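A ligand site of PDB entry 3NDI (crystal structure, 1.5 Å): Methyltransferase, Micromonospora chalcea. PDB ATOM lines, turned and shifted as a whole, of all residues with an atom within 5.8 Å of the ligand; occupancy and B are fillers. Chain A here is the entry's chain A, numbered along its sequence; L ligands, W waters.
OG1 of Thr 352 lies within hydrogen-bond range of O6 of the ligand (3.4 Å). An oxygen (O7) of the ligand lies within hydrogen-bond range of the backbone NH (N) of Thr 351 (3.0 Å). The side-chain amino group (NZ) of Lys 330 is in salt-bridge range of an oxygen (O1) of the ligand (2.9 Å). The side-chain carboxylate of Asp 350 sits at hydrogen-bond distance from an oxygen (O6) of the ligand (2.5 Å). O2 of the ligand is in hydrogen-bond range of OH of Tyr 80, 2.5 Å away. An oxygen (O2) of the ligand sits at hydrogen-bond distance from a ring nitrogen (NE2) of His 388 (2.9 Å). ND2 of Asn 387 is in hydrogen-bond range of O1 of the ligand, 2.9 Å away. An oxygen (O7) of the ligand is in hydrogen-bond range of the side-chain hydroxyl of Thr 351. An oxygen (O6) of the ligand lies within hydrogen-bond range of the side-chain amino group of Lys 355 (2.8 Å). NZ of Lys 395 is in hydrogen-bond range of O8 of the ligand (2.8 Å).
N of Ala 370 lies within hydrogen-bond range of O of Asp 350. The backbone NH of Ala 327 lies within hydrogen-bond range of the side-chain carboxylate of Asp 350 (2.8 Å). N of Gly 326 lies within hydrogen-bond range of O of Tyr 349 (2.8 Å). The side-chain carboxylate of Glu 391 is in hydrogen-bond range of the side-chain hydroxyl of Ser 85 (2.7 Å). The backbone NH of Ala 385 lies within hydrogen-bond range of the backbone carbonyl oxygen of Tyr 325, 3.1 Å away. The side-chain amide nitrogen (ND2) of Asn 387 sits at hydrogen-bond distance from a ring nitrogen (ND1) of His 256, 3.3 Å away. NE2 of His 388 is in hydrogen-bond range of ND2 of Asn 387 (3.2 Å). O of Ala 327 lies within hydrogen-bond range of NZ of Lys 355 (2.7 Å).
His 256 touches the ligand (CE1 to O2, 3.5 Å). Gly 326 touches the ligand. Ala 327 touches the ligand (O to O6, 3.7 Å). Thr 328 touches the ligand. CB of Ala 385 touches O5 of the ligand, at 3.9 Å. Glu 391 touches the ligand (OE1 to C9, 3.6 Å). CG1 of Ile 392 touches O8 of the ligand, at 3.4 Å. Along chain A the residues within 4 Å of the ligand span positions 80 to 395.
Water W7 bridges O3 of the ligand and N of Ala 329. Water W4 lies within hydrogen-bond range of an oxygen (O3) of the ligand, the side-chain amino group (NZ) of Lys 330, the side-chain hydroxyl (OH) of Tyr 224 and the backbone NH (N) of Ala 329. Water W2 lies within hydrogen-bond range of OH of Tyr 325 (2.8 Å), N2 of the ligand (2.8 Å) and NZ of Lys 395 (3.3 Å). Water W5 lies within hydrogen-bond range of O2 of the ligand (2.9 Å), NE2 of His 388 (3.4 Å) and OH of Tyr 80 (3.4 Å). Water W3 lies within hydrogen-bond range of the backbone carbonyl oxygen of Gly 84 (2.7 Å), the side-chain hydroxyl of Thr 351 (2.8 Å) and a nitrogen (N2) of the ligand (3.5 Å).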
ATOM      1  N   TYR A  80     -15.905 -19.588  10.053  1.00  0.00           N
ATOM      2  CA  TYR A  80     -14.850 -18.606  10.349  1.00  0.00           C
ATOM      3  C   TYR A  80     -14.017 -19.042  11.536  1.00  0.00           C
ATOM      4  O   TYR A  80     -14.569 -19.322  12.604  1.00  0.00           O
ATOM      5  CB  TYR A  80     -15.494 -17.278  10.766  1.00  0.00           C
ATOM      6  CG  TYR A  80     -14.507 -16.180  11.023  1.00  0.00           C
ATOM      7  CD1 TYR A  80     -13.630 -15.762  10.015  1.00  0.00           C
ATOM      8  CD2 TYR A  80     -14.418 -15.563  12.267  1.00  0.00           C
ATOM      9  CE1 TYR A  80     -12.715 -14.744  10.191  1.00  0.00           C
ATOM     10  CE2 TYR A  80     -13.501 -14.549  12.473  1.00  0.00           C
ATOM     11  CZ  TYR A  80     -12.658 -14.166  11.441  1.00  0.00           C
ATOM     12  OH  TYR A  80     -11.768 -13.134  11.624  1.00  0.00           O
ATOM     13  N   GLY A  84      -7.117 -17.923  12.632  1.00  0.00           N
ATOM     14  CA  GLY A  84      -6.384 -17.855  11.373  1.00  0.00           C
ATOM     15  C   GLY A  84      -5.485 -16.653  11.155  1.00  0.00           C
ATOM     16  O   GLY A  84      -4.682 -16.615  10.213  1.00  0.00           O
ATOM     17  N   SER A  85      -5.598 -15.660  12.035  1.00  0.00           N
ATOM     18  CA  SER A  85      -4.788 -14.436  11.899  1.00  0.00           C
ATOM     19  C   SER A  85      -3.816 -14.316  13.062  1.00  0.00           C
ATOM     20  O   SER A  85      -4.209 -14.334  14.217  1.00  0.00           O
ATOM     21  CB  SER A  85      -5.686 -13.191  11.918  1.00  0.00           C
ATOM     22  OG  SER A  85      -4.899 -12.018  12.070  1.00  0.00           O
ATOM     23  N   SER A  86      -2.519 -14.177  12.764  1.00  0.00           N
ATOM     24  CA  SER A  86      -1.529 -14.038  13.838  1.00  0.00           C
ATOM     25  C   SER A  86      -1.704 -12.694  14.532  1.00  0.00           C
ATOM     26  O   SER A  86      -1.550 -12.607  15.759  1.00  0.00           O
ATOM     27  CB  SER A  86      -0.125 -14.171  13.237  1.00  0.00           C
ATOM     28  OG  SER A  86       0.142 -13.110  12.330  1.00  0.00           O
ATOM     29  N   TYR A 224     -22.922  -6.822   5.527  1.00  0.00           N
ATOM     30  CA  TYR A 224     -23.313  -8.170   5.058  1.00  0.00           C
ATOM     31  C   TYR A 224     -24.236  -8.789   6.119  1.00  0.00           C
ATOM     32  O   TYR A 224     -24.459  -8.184   7.165  1.00  0.00           O
ATOM     33  CB  TYR A 224     -22.105  -9.016   4.642  1.00  0.00           C
ATOM     34  CG  TYR A 224     -21.052  -9.325   5.713  1.00  0.00           C
ATOM     35  CD1 TYR A 224     -21.131 -10.512   6.469  1.00  0.00           C
ATOM     36  CD2 TYR A 224     -19.995  -8.447   5.947  1.00  0.00           C
ATOM     37  CE1 TYR A 224     -20.152 -10.822   7.421  1.00  0.00           C
ATOM     38  CE2 TYR A 224     -19.036  -8.781   6.870  1.00  0.00           C
ATOM     39  CZ  TYR A 224     -19.118  -9.925   7.644  1.00  0.00           C
ATOM     40  OH  TYR A 224     -18.171 -10.300   8.583  1.00  0.00           O
ATOM     41  N   HIS A 256      -9.476  -5.113  11.836  1.00  0.00           N
ATOM     42  CA  HIS A 256     -10.694  -5.230  11.063  1.00  0.00           C
ATOM     43  C   HIS A 256     -11.142  -4.014  10.280  1.00  0.00           C
ATOM     44  O   HIS A 256     -12.350  -3.798  10.176  1.00  0.00           O
ATOM     45  CB  HIS A 256     -11.791  -5.799  11.954  1.00  0.00           C
ATOM     46  CG  HIS A 256     -11.554  -7.253  12.226  1.00  0.00           C
ATOM     47  ND1 HIS A 256     -11.566  -8.187  11.213  1.00  0.00           N
ATOM     48  CD2 HIS A 256     -11.300  -7.924  13.380  1.00  0.00           C
ATOM     49  CE1 HIS A 256     -11.294  -9.378  11.726  1.00  0.00           C
ATOM     50  NE2 HIS A 256     -11.158  -9.252  13.035  1.00  0.00           N
ATOM     51  N   TYR A 325      -7.802 -12.869  -2.979  1.00  0.00           N
ATOM     52  CA  TYR A 325      -7.124 -13.338  -1.795  1.00  0.00           C
ATOM     53  C   TYR A 325      -7.920 -13.064  -0.528  1.00  0.00           C
ATOM     54  O   TYR A 325      -8.153 -11.890  -0.198  1.00  0.00           O
ATOM     55  CB  TYR A 325      -5.762 -12.681  -1.713  1.00  0.00           C
ATOM     56  CG  TYR A 325      -4.765 -13.486  -0.916  1.00  0.00           C
ATOM     57  CD1 TYR A 325      -4.965 -13.706   0.458  1.00  0.00           C
ATOM     58  CD2 TYR A 325      -3.638 -14.032  -1.536  1.00  0.00           C
ATOM     59  CE1 TYR A 325      -4.012 -14.429   1.199  1.00  0.00           C
ATOM     60  CE2 TYR A 325      -2.705 -14.764  -0.795  1.00  0.00           C
ATOM     61  CZ  TYR A 325      -2.899 -14.938   0.557  1.00  0.00           C
ATOM     62  OH  TYR A 325      -1.941 -15.690   1.204  1.00  0.00           O
ATOM     63  N   GLY A 326      -8.360 -14.131   0.148  1.00  0.00           N
ATOM     64  CA  GLY A 326      -9.091 -14.065   1.407  1.00  0.00           C
ATOM     65  C   GLY A 326     -10.555 -14.279   1.117  1.00  0.00           C
ATOM     66  O   GLY A 326     -11.234 -13.398   0.574  1.00  0.00           O
ATOM     67  N   ALA A 327     -11.094 -15.451   1.441  1.00  0.00           N
ATOM     68  CA  ALA A 327     -12.546 -15.701   1.345  1.00  0.00           C
ATOM     69  C   ALA A 327     -13.291 -15.167   2.567  1.00  0.00           C
ATOM     70  O   ALA A 327     -13.955 -15.924   3.272  1.00  0.00           O
ATOM     71  CB  ALA A 327     -12.859 -17.231   1.105  1.00  0.00           C
ATOM     72  N   THR A 328     -13.185 -13.856   2.775  1.00  0.00           N
ATOM     73  CA  THR A 328     -13.891 -13.192   3.866  1.00  0.00           C
ATOM     74  C   THR A 328     -15.396 -13.311   3.659  1.00  0.00           C
ATOM     75  O   THR A 328     -15.925 -13.413   2.535  1.00  0.00           O
ATOM     76  CB  THR A 328     -13.558 -11.674   3.843  1.00  0.00           C
ATOM     77  OG1 THR A 328     -13.967 -11.181   2.562  1.00  0.00           O
ATOM     78  CG2 THR A 328     -12.014 -11.494   4.002  1.00  0.00           C
ATOM     79  N   ALA A 329     -16.122 -13.275   4.756  1.00  0.00           N
ATOM     80  CA  ALA A 329     -17.568 -13.048   4.691  1.00  0.00           C
ATOM     81  C   ALA A 329     -17.904 -11.730   3.960  1.00  0.00           C
ATOM     82  O   ALA A 329     -18.814 -11.622   3.130  1.00  0.00           O
ATOM     83  CB  ALA A 329     -18.164 -13.056   6.111  1.00  0.00           C
ATOM     84  N   LYS A 330     -17.082 -10.713   4.223  1.00  0.00           N
ATOM     85  CA  LYS A 330     -17.228  -9.402   3.593  1.00  0.00           C
ATOM     86  C   LYS A 330     -17.303  -9.501   2.070  1.00  0.00           C
ATOM     87  O   LYS A 330     -18.014  -8.738   1.423  1.00  0.00           O
ATOM     88  CB  LYS A 330     -16.001  -8.507   3.900  1.00  0.00           C
ATOM     89  CG  LYS A 330     -15.846  -8.056   5.381  1.00  0.00           C
ATOM     90  CD  LYS A 330     -14.627  -7.080   5.608  1.00  0.00           C
ATOM     91  CE  LYS A 330     -13.296  -7.800   5.616  1.00  0.00           C
ATOM     92  NZ  LYS A 330     -13.384  -8.754   6.754  1.00  0.00           N
ATOM     93  N   TYR A 349      -7.976 -17.397  -2.870  1.00  0.00           N
ATOM     94  CA  TYR A 349      -7.039 -18.167  -2.030  1.00  0.00           C
ATOM     95  C   TYR A 349      -7.340 -17.913  -0.542  1.00  0.00           C
ATOM     96  O   TYR A 349      -7.569 -16.759  -0.181  1.00  0.00           O
ATOM     97  CB  TYR A 349      -5.551 -17.855  -2.411  1.00  0.00           C
ATOM     98  CG  TYR A 349      -5.375 -18.297  -3.834  1.00  0.00           C
ATOM     99  CD1 TYR A 349      -5.137 -19.636  -4.109  1.00  0.00           C
ATOM    100  CD2 TYR A 349      -5.515 -17.405  -4.898  1.00  0.00           C
ATOM    101  CE1 TYR A 349      -4.998 -20.090  -5.400  1.00  0.00           C
ATOM    102  CE2 TYR A 349      -5.385 -17.838  -6.197  1.00  0.00           C
ATOM    103  CZ  TYR A 349      -5.115 -19.163  -6.432  1.00  0.00           C
ATOM    104  OH  TYR A 349      -4.996 -19.626  -7.724  1.00  0.00           O
ATOM    105  N   ASP A 350      -7.379 -18.966   0.268  1.00  0.00           N
ATOM    106  CA  ASP A 350      -7.799 -18.852   1.667  1.00  0.00           C
ATOM    107  C   ASP A 350      -7.200 -19.947   2.540  1.00  0.00           C
ATOM    108  O   ASP A 350      -7.148 -21.106   2.120  1.00  0.00           O
ATOM    109  CB  ASP A 350      -9.326 -18.821   1.797  1.00  0.00           C
ATOM    110  CG  ASP A 350      -9.809 -18.407   3.171  1.00  0.00           C
ATOM    111  OD1 ASP A 350     -10.112 -17.197   3.340  1.00  0.00           O
ATOM    112  OD2 ASP A 350      -9.933 -19.287   4.037  1.00  0.00           O
ATOM    113  N   THR A 351      -6.793 -19.586   3.758  1.00  0.00           N
ATOM    114  CA  THR A 351      -6.154 -20.559   4.627  1.00  0.00           C
ATOM    115  C   THR A 351      -7.158 -21.446   5.395  1.00  0.00           C
ATOM    116  O   THR A 351      -6.685 -22.285   6.163  1.00  0.00           O
ATOM    117  CB  THR A 351      -5.253 -19.853   5.638  1.00  0.00           C
ATOM    118  OG1 THR A 351      -6.006 -18.841   6.324  1.00  0.00           O
ATOM    119  CG2 THR A 351      -4.074 -19.189   4.927  1.00  0.00           C
ATOM    120  N   THR A 352      -8.464 -21.246   5.255  1.00  0.00           N
ATOM    121  CA  THR A 352      -9.410 -21.997   6.094  1.00  0.00           C
ATOM    122  C   THR A 352      -9.775 -23.328   5.408  1.00  0.00           C
ATOM    123  O   THR A 352     -10.352 -23.363   4.320  1.00  0.00           O
ATOM    124  CB  THR A 352     -10.689 -21.168   6.324  1.00  0.00           C
ATOM    125  OG1 THR A 352     -10.379 -19.793   6.621  1.00  0.00           O
ATOM    126  CG2 THR A 352     -11.463 -21.801   7.477  1.00  0.00           C
ATOM    127  N   LYS A 355     -13.244 -23.882   3.934  1.00  0.00           N
ATOM    128  CA  LYS A 355     -13.678 -23.060   2.793  1.00  0.00           C
ATOM    129  C   LYS A 355     -13.022 -23.563   1.527  1.00  0.00           C
ATOM    130  O   LYS A 355     -13.493 -23.264   0.421  1.00  0.00           O
ATOM    131  CB  LYS A 355     -13.237 -21.588   2.966  1.00  0.00           C
ATOM    132  CG  LYS A 355     -13.917 -20.990   4.213  1.00  0.00           C
ATOM    133  CD  LYS A 355     -13.620 -19.496   4.329  1.00  0.00           C
ATOM    134  CE  LYS A 355     -14.275 -18.843   5.554  1.00  0.00           C
ATOM    135  NZ  LYS A 355     -13.836 -17.404   5.539  1.00  0.00           N
ATOM    136  N   ALA A 370      -4.345 -21.290   0.384  1.00  0.00           N
ATOM    137  CA  ALA A 370      -3.397 -20.216   0.167  1.00  0.00           C
ATOM    138  C   ALA A 370      -2.061 -20.780  -0.297  1.00  0.00           C
ATOM    139  O   ALA A 370      -1.293 -20.088  -0.966  1.00  0.00           O
ATOM    140  CB  ALA A 370      -3.157 -19.445   1.473  1.00  0.00           C
ATOM    141  N   ALA A 385      -9.207  -9.731   1.723  1.00  0.00           N
ATOM    142  CA  ALA A 385      -8.817  -9.567   3.147  1.00  0.00           C
ATOM    143  C   ALA A 385      -7.915  -8.349   3.371  1.00  0.00           C
ATOM    144  O   ALA A 385      -6.779  -8.435   3.851  1.00  0.00           O
ATOM    145  CB  ALA A 385      -8.104 -10.878   3.583  1.00  0.00           C
ATOM    146  N   ASN A 387      -8.249  -5.932   5.371  1.00  0.00           N
ATOM    147  CA  ASN A 387      -8.065  -5.616   6.784  1.00  0.00           C
ATOM    148  C   ASN A 387      -6.882  -6.410   7.319  1.00  0.00           C
ATOM    149  O   ASN A 387      -6.386  -6.094   8.405  1.00  0.00           O
ATOM    150  CB  ASN A 387      -9.354  -5.965   7.535  1.00  0.00           C
ATOM    151  CG  ASN A 387      -9.866  -7.368   7.241  1.00  0.00           C
ATOM    152  OD1 ASN A 387     -10.102  -7.700   6.089  1.00  0.00           O
ATOM    153  ND2 ASN A 387     -10.063  -8.175   8.276  1.00  0.00           N
ATOM    154  N   HIS A 388      -6.425  -7.432   6.587  1.00  0.00           N
ATOM    155  CA  HIS A 388      -5.263  -8.198   6.998  1.00  0.00           C
ATOM    156  C   HIS A 388      -4.063  -7.962   6.079  1.00  0.00           C
ATOM    157  O   HIS A 388      -3.184  -8.837   5.956  1.00  0.00           O
ATOM    158  CB  HIS A 388      -5.610  -9.692   6.971  1.00  0.00           C
ATOM    159  CG  HIS A 388      -6.663 -10.127   7.929  1.00  0.00           C
ATOM    160  ND1 HIS A 388      -6.411 -10.151   9.282  1.00  0.00           N
ATOM    161  CD2 HIS A 388      -7.934 -10.546   7.741  1.00  0.00           C
ATOM    162  CE1 HIS A 388      -7.495 -10.611   9.889  1.00  0.00           C
ATOM    163  NE2 HIS A 388      -8.444 -10.842   8.985  1.00  0.00           N
ATOM    164  N   GLU A 391      -0.300  -8.549   7.312  1.00  0.00           N
ATOM    165  CA  GLU A 391       0.009  -9.923   7.666  1.00  0.00           C
ATOM    166  C   GLU A 391       0.102 -10.784   6.406  1.00  0.00           C
ATOM    167  O   GLU A 391       0.992 -11.641   6.284  1.00  0.00           O
ATOM    168  CB  GLU A 391      -1.132 -10.445   8.556  1.00  0.00           C
ATOM    169  CG  GLU A 391      -0.911 -11.889   8.988  1.00  0.00           C
ATOM    170  CD  GLU A 391      -1.936 -12.392   9.998  1.00  0.00           C
ATOM    171  OE1 GLU A 391      -2.060 -13.629  10.098  1.00  0.00           O
ATOM    172  OE2 GLU A 391      -2.623 -11.583  10.659  1.00  0.00           O
ATOM    173  N   ILE A 392      -0.825 -10.575   5.487  1.00  0.00           N
ATOM    174  CA  ILE A 392      -0.814 -11.290   4.227  1.00  0.00           C
ATOM    175  C   ILE A 392       0.356 -10.904   3.336  1.00  0.00           C
ATOM    176  O   ILE A 392       1.065 -11.785   2.848  1.00  0.00           O
ATOM    177  CB  ILE A 392      -2.141 -11.161   3.442  1.00  0.00           C
ATOM    178  CG1 ILE A 392      -3.241 -11.958   4.182  1.00  0.00           C
ATOM    179  CG2 ILE A 392      -1.965 -11.696   2.016  1.00  0.00           C
ATOM    180  CD1 ILE A 392      -4.717 -11.665   3.733  1.00  0.00           C
ATOM    181  N   LYS A 395       3.608 -12.433   4.184  1.00  0.00           N
ATOM    182  CA  LYS A 395       3.791 -13.849   3.912  1.00  0.00           C
ATOM    183  C   LYS A 395       3.861 -14.050   2.403  1.00  0.00           C
ATOM    184  O   LYS A 395       4.191 -15.127   1.937  1.00  0.00           O
ATOM    185  CB  LYS A 395       2.591 -14.673   4.411  1.00  0.00           C
ATOM    186  CG  LYS A 395       2.415 -14.623   5.909  1.00  0.00           C
ATOM    187  CD  LYS A 395       1.457 -15.695   6.388  1.00  0.00           C
ATOM    188  CE  LYS A 395       0.031 -15.191   6.240  1.00  0.00           C
ATOM    189  NZ  LYS A 395      -0.852 -16.322   6.661  1.00  0.00           N
HETATM  190  P1  LIG L   1     -11.819 -11.821   8.208  1.00  0.00           P
HETATM  191  O1  LIG L   1     -11.281 -10.649   7.417  1.00  0.00           O
HETATM  192  O2  LIG L   1     -10.979 -12.069   9.460  1.00  0.00           O
HETATM  193  O3  LIG L   1     -13.308 -11.828   8.517  1.00  0.00           O
HETATM  194  O4  LIG L   1     -11.508 -13.048   7.202  1.00  0.00           O
HETATM  195  C1  LIG L   1     -10.236 -13.294   6.645  1.00  0.00           C
HETATM  196  C2  LIG L   1     -10.325 -14.474   5.683  1.00  0.00           C
HETATM  197  O5  LIG L   1      -9.068 -14.396   5.033  1.00  0.00           O
HETATM  198  C3  LIG L   1     -10.347 -15.817   6.426  1.00  0.00           C
HETATM  199  O6  LIG L   1     -11.147 -16.654   5.571  1.00  0.00           O
HETATM  200  C4  LIG L   1      -8.899 -16.267   6.472  1.00  0.00           C
HETATM  201  C5  LIG L   1      -8.269 -15.558   5.285  1.00  0.00           C
HETATM  202  N1  LIG L   1      -6.836 -15.302   5.490  1.00  0.00           N
HETATM  203  C6  LIG L   1      -5.880 -15.909   4.764  1.00  0.00           C
HETATM  204  O7  LIG L   1      -6.259 -16.681   3.861  1.00  0.00           O
HETATM  205  N2  LIG L   1      -4.583 -15.622   5.027  1.00  0.00           N
HETATM  206  C7  LIG L   1      -4.177 -14.814   6.044  1.00  0.00           C
HETATM  207  O8  LIG L   1      -2.967 -14.595   6.251  1.00  0.00           O
HETATM  208  C8  LIG L   1      -5.151 -14.190   6.803  1.00  0.00           C
HETATM  209  C9  LIG L   1      -4.855 -13.220   7.929  1.00  0.00           C
HETATM  210  C10 LIG L   1      -6.485 -14.457   6.497  1.00  0.00           C
HETATM  211  O   HOH W   1     -14.962 -11.826  10.614  1.00  0.00           O
HETATM  212  O   HOH W   2      -2.331 -16.682   3.746  1.00  0.00           O
HETATM  213  O   HOH W   3      -4.027 -17.604   7.803  1.00  0.00           O
HETATM  214  O   HOH W   4     -15.464 -10.783   7.080  1.00  0.00           O
HETATM  215  O   HOH W   5      -8.948 -14.081   9.883  1.00  0.00           O
HETATM  216  O   HOH W   6      -9.480 -16.949   9.589  1.00  0.00           O
HETATM  217  O   HOH W   7     -15.125 -13.698   7.554  1.00  0.00           O
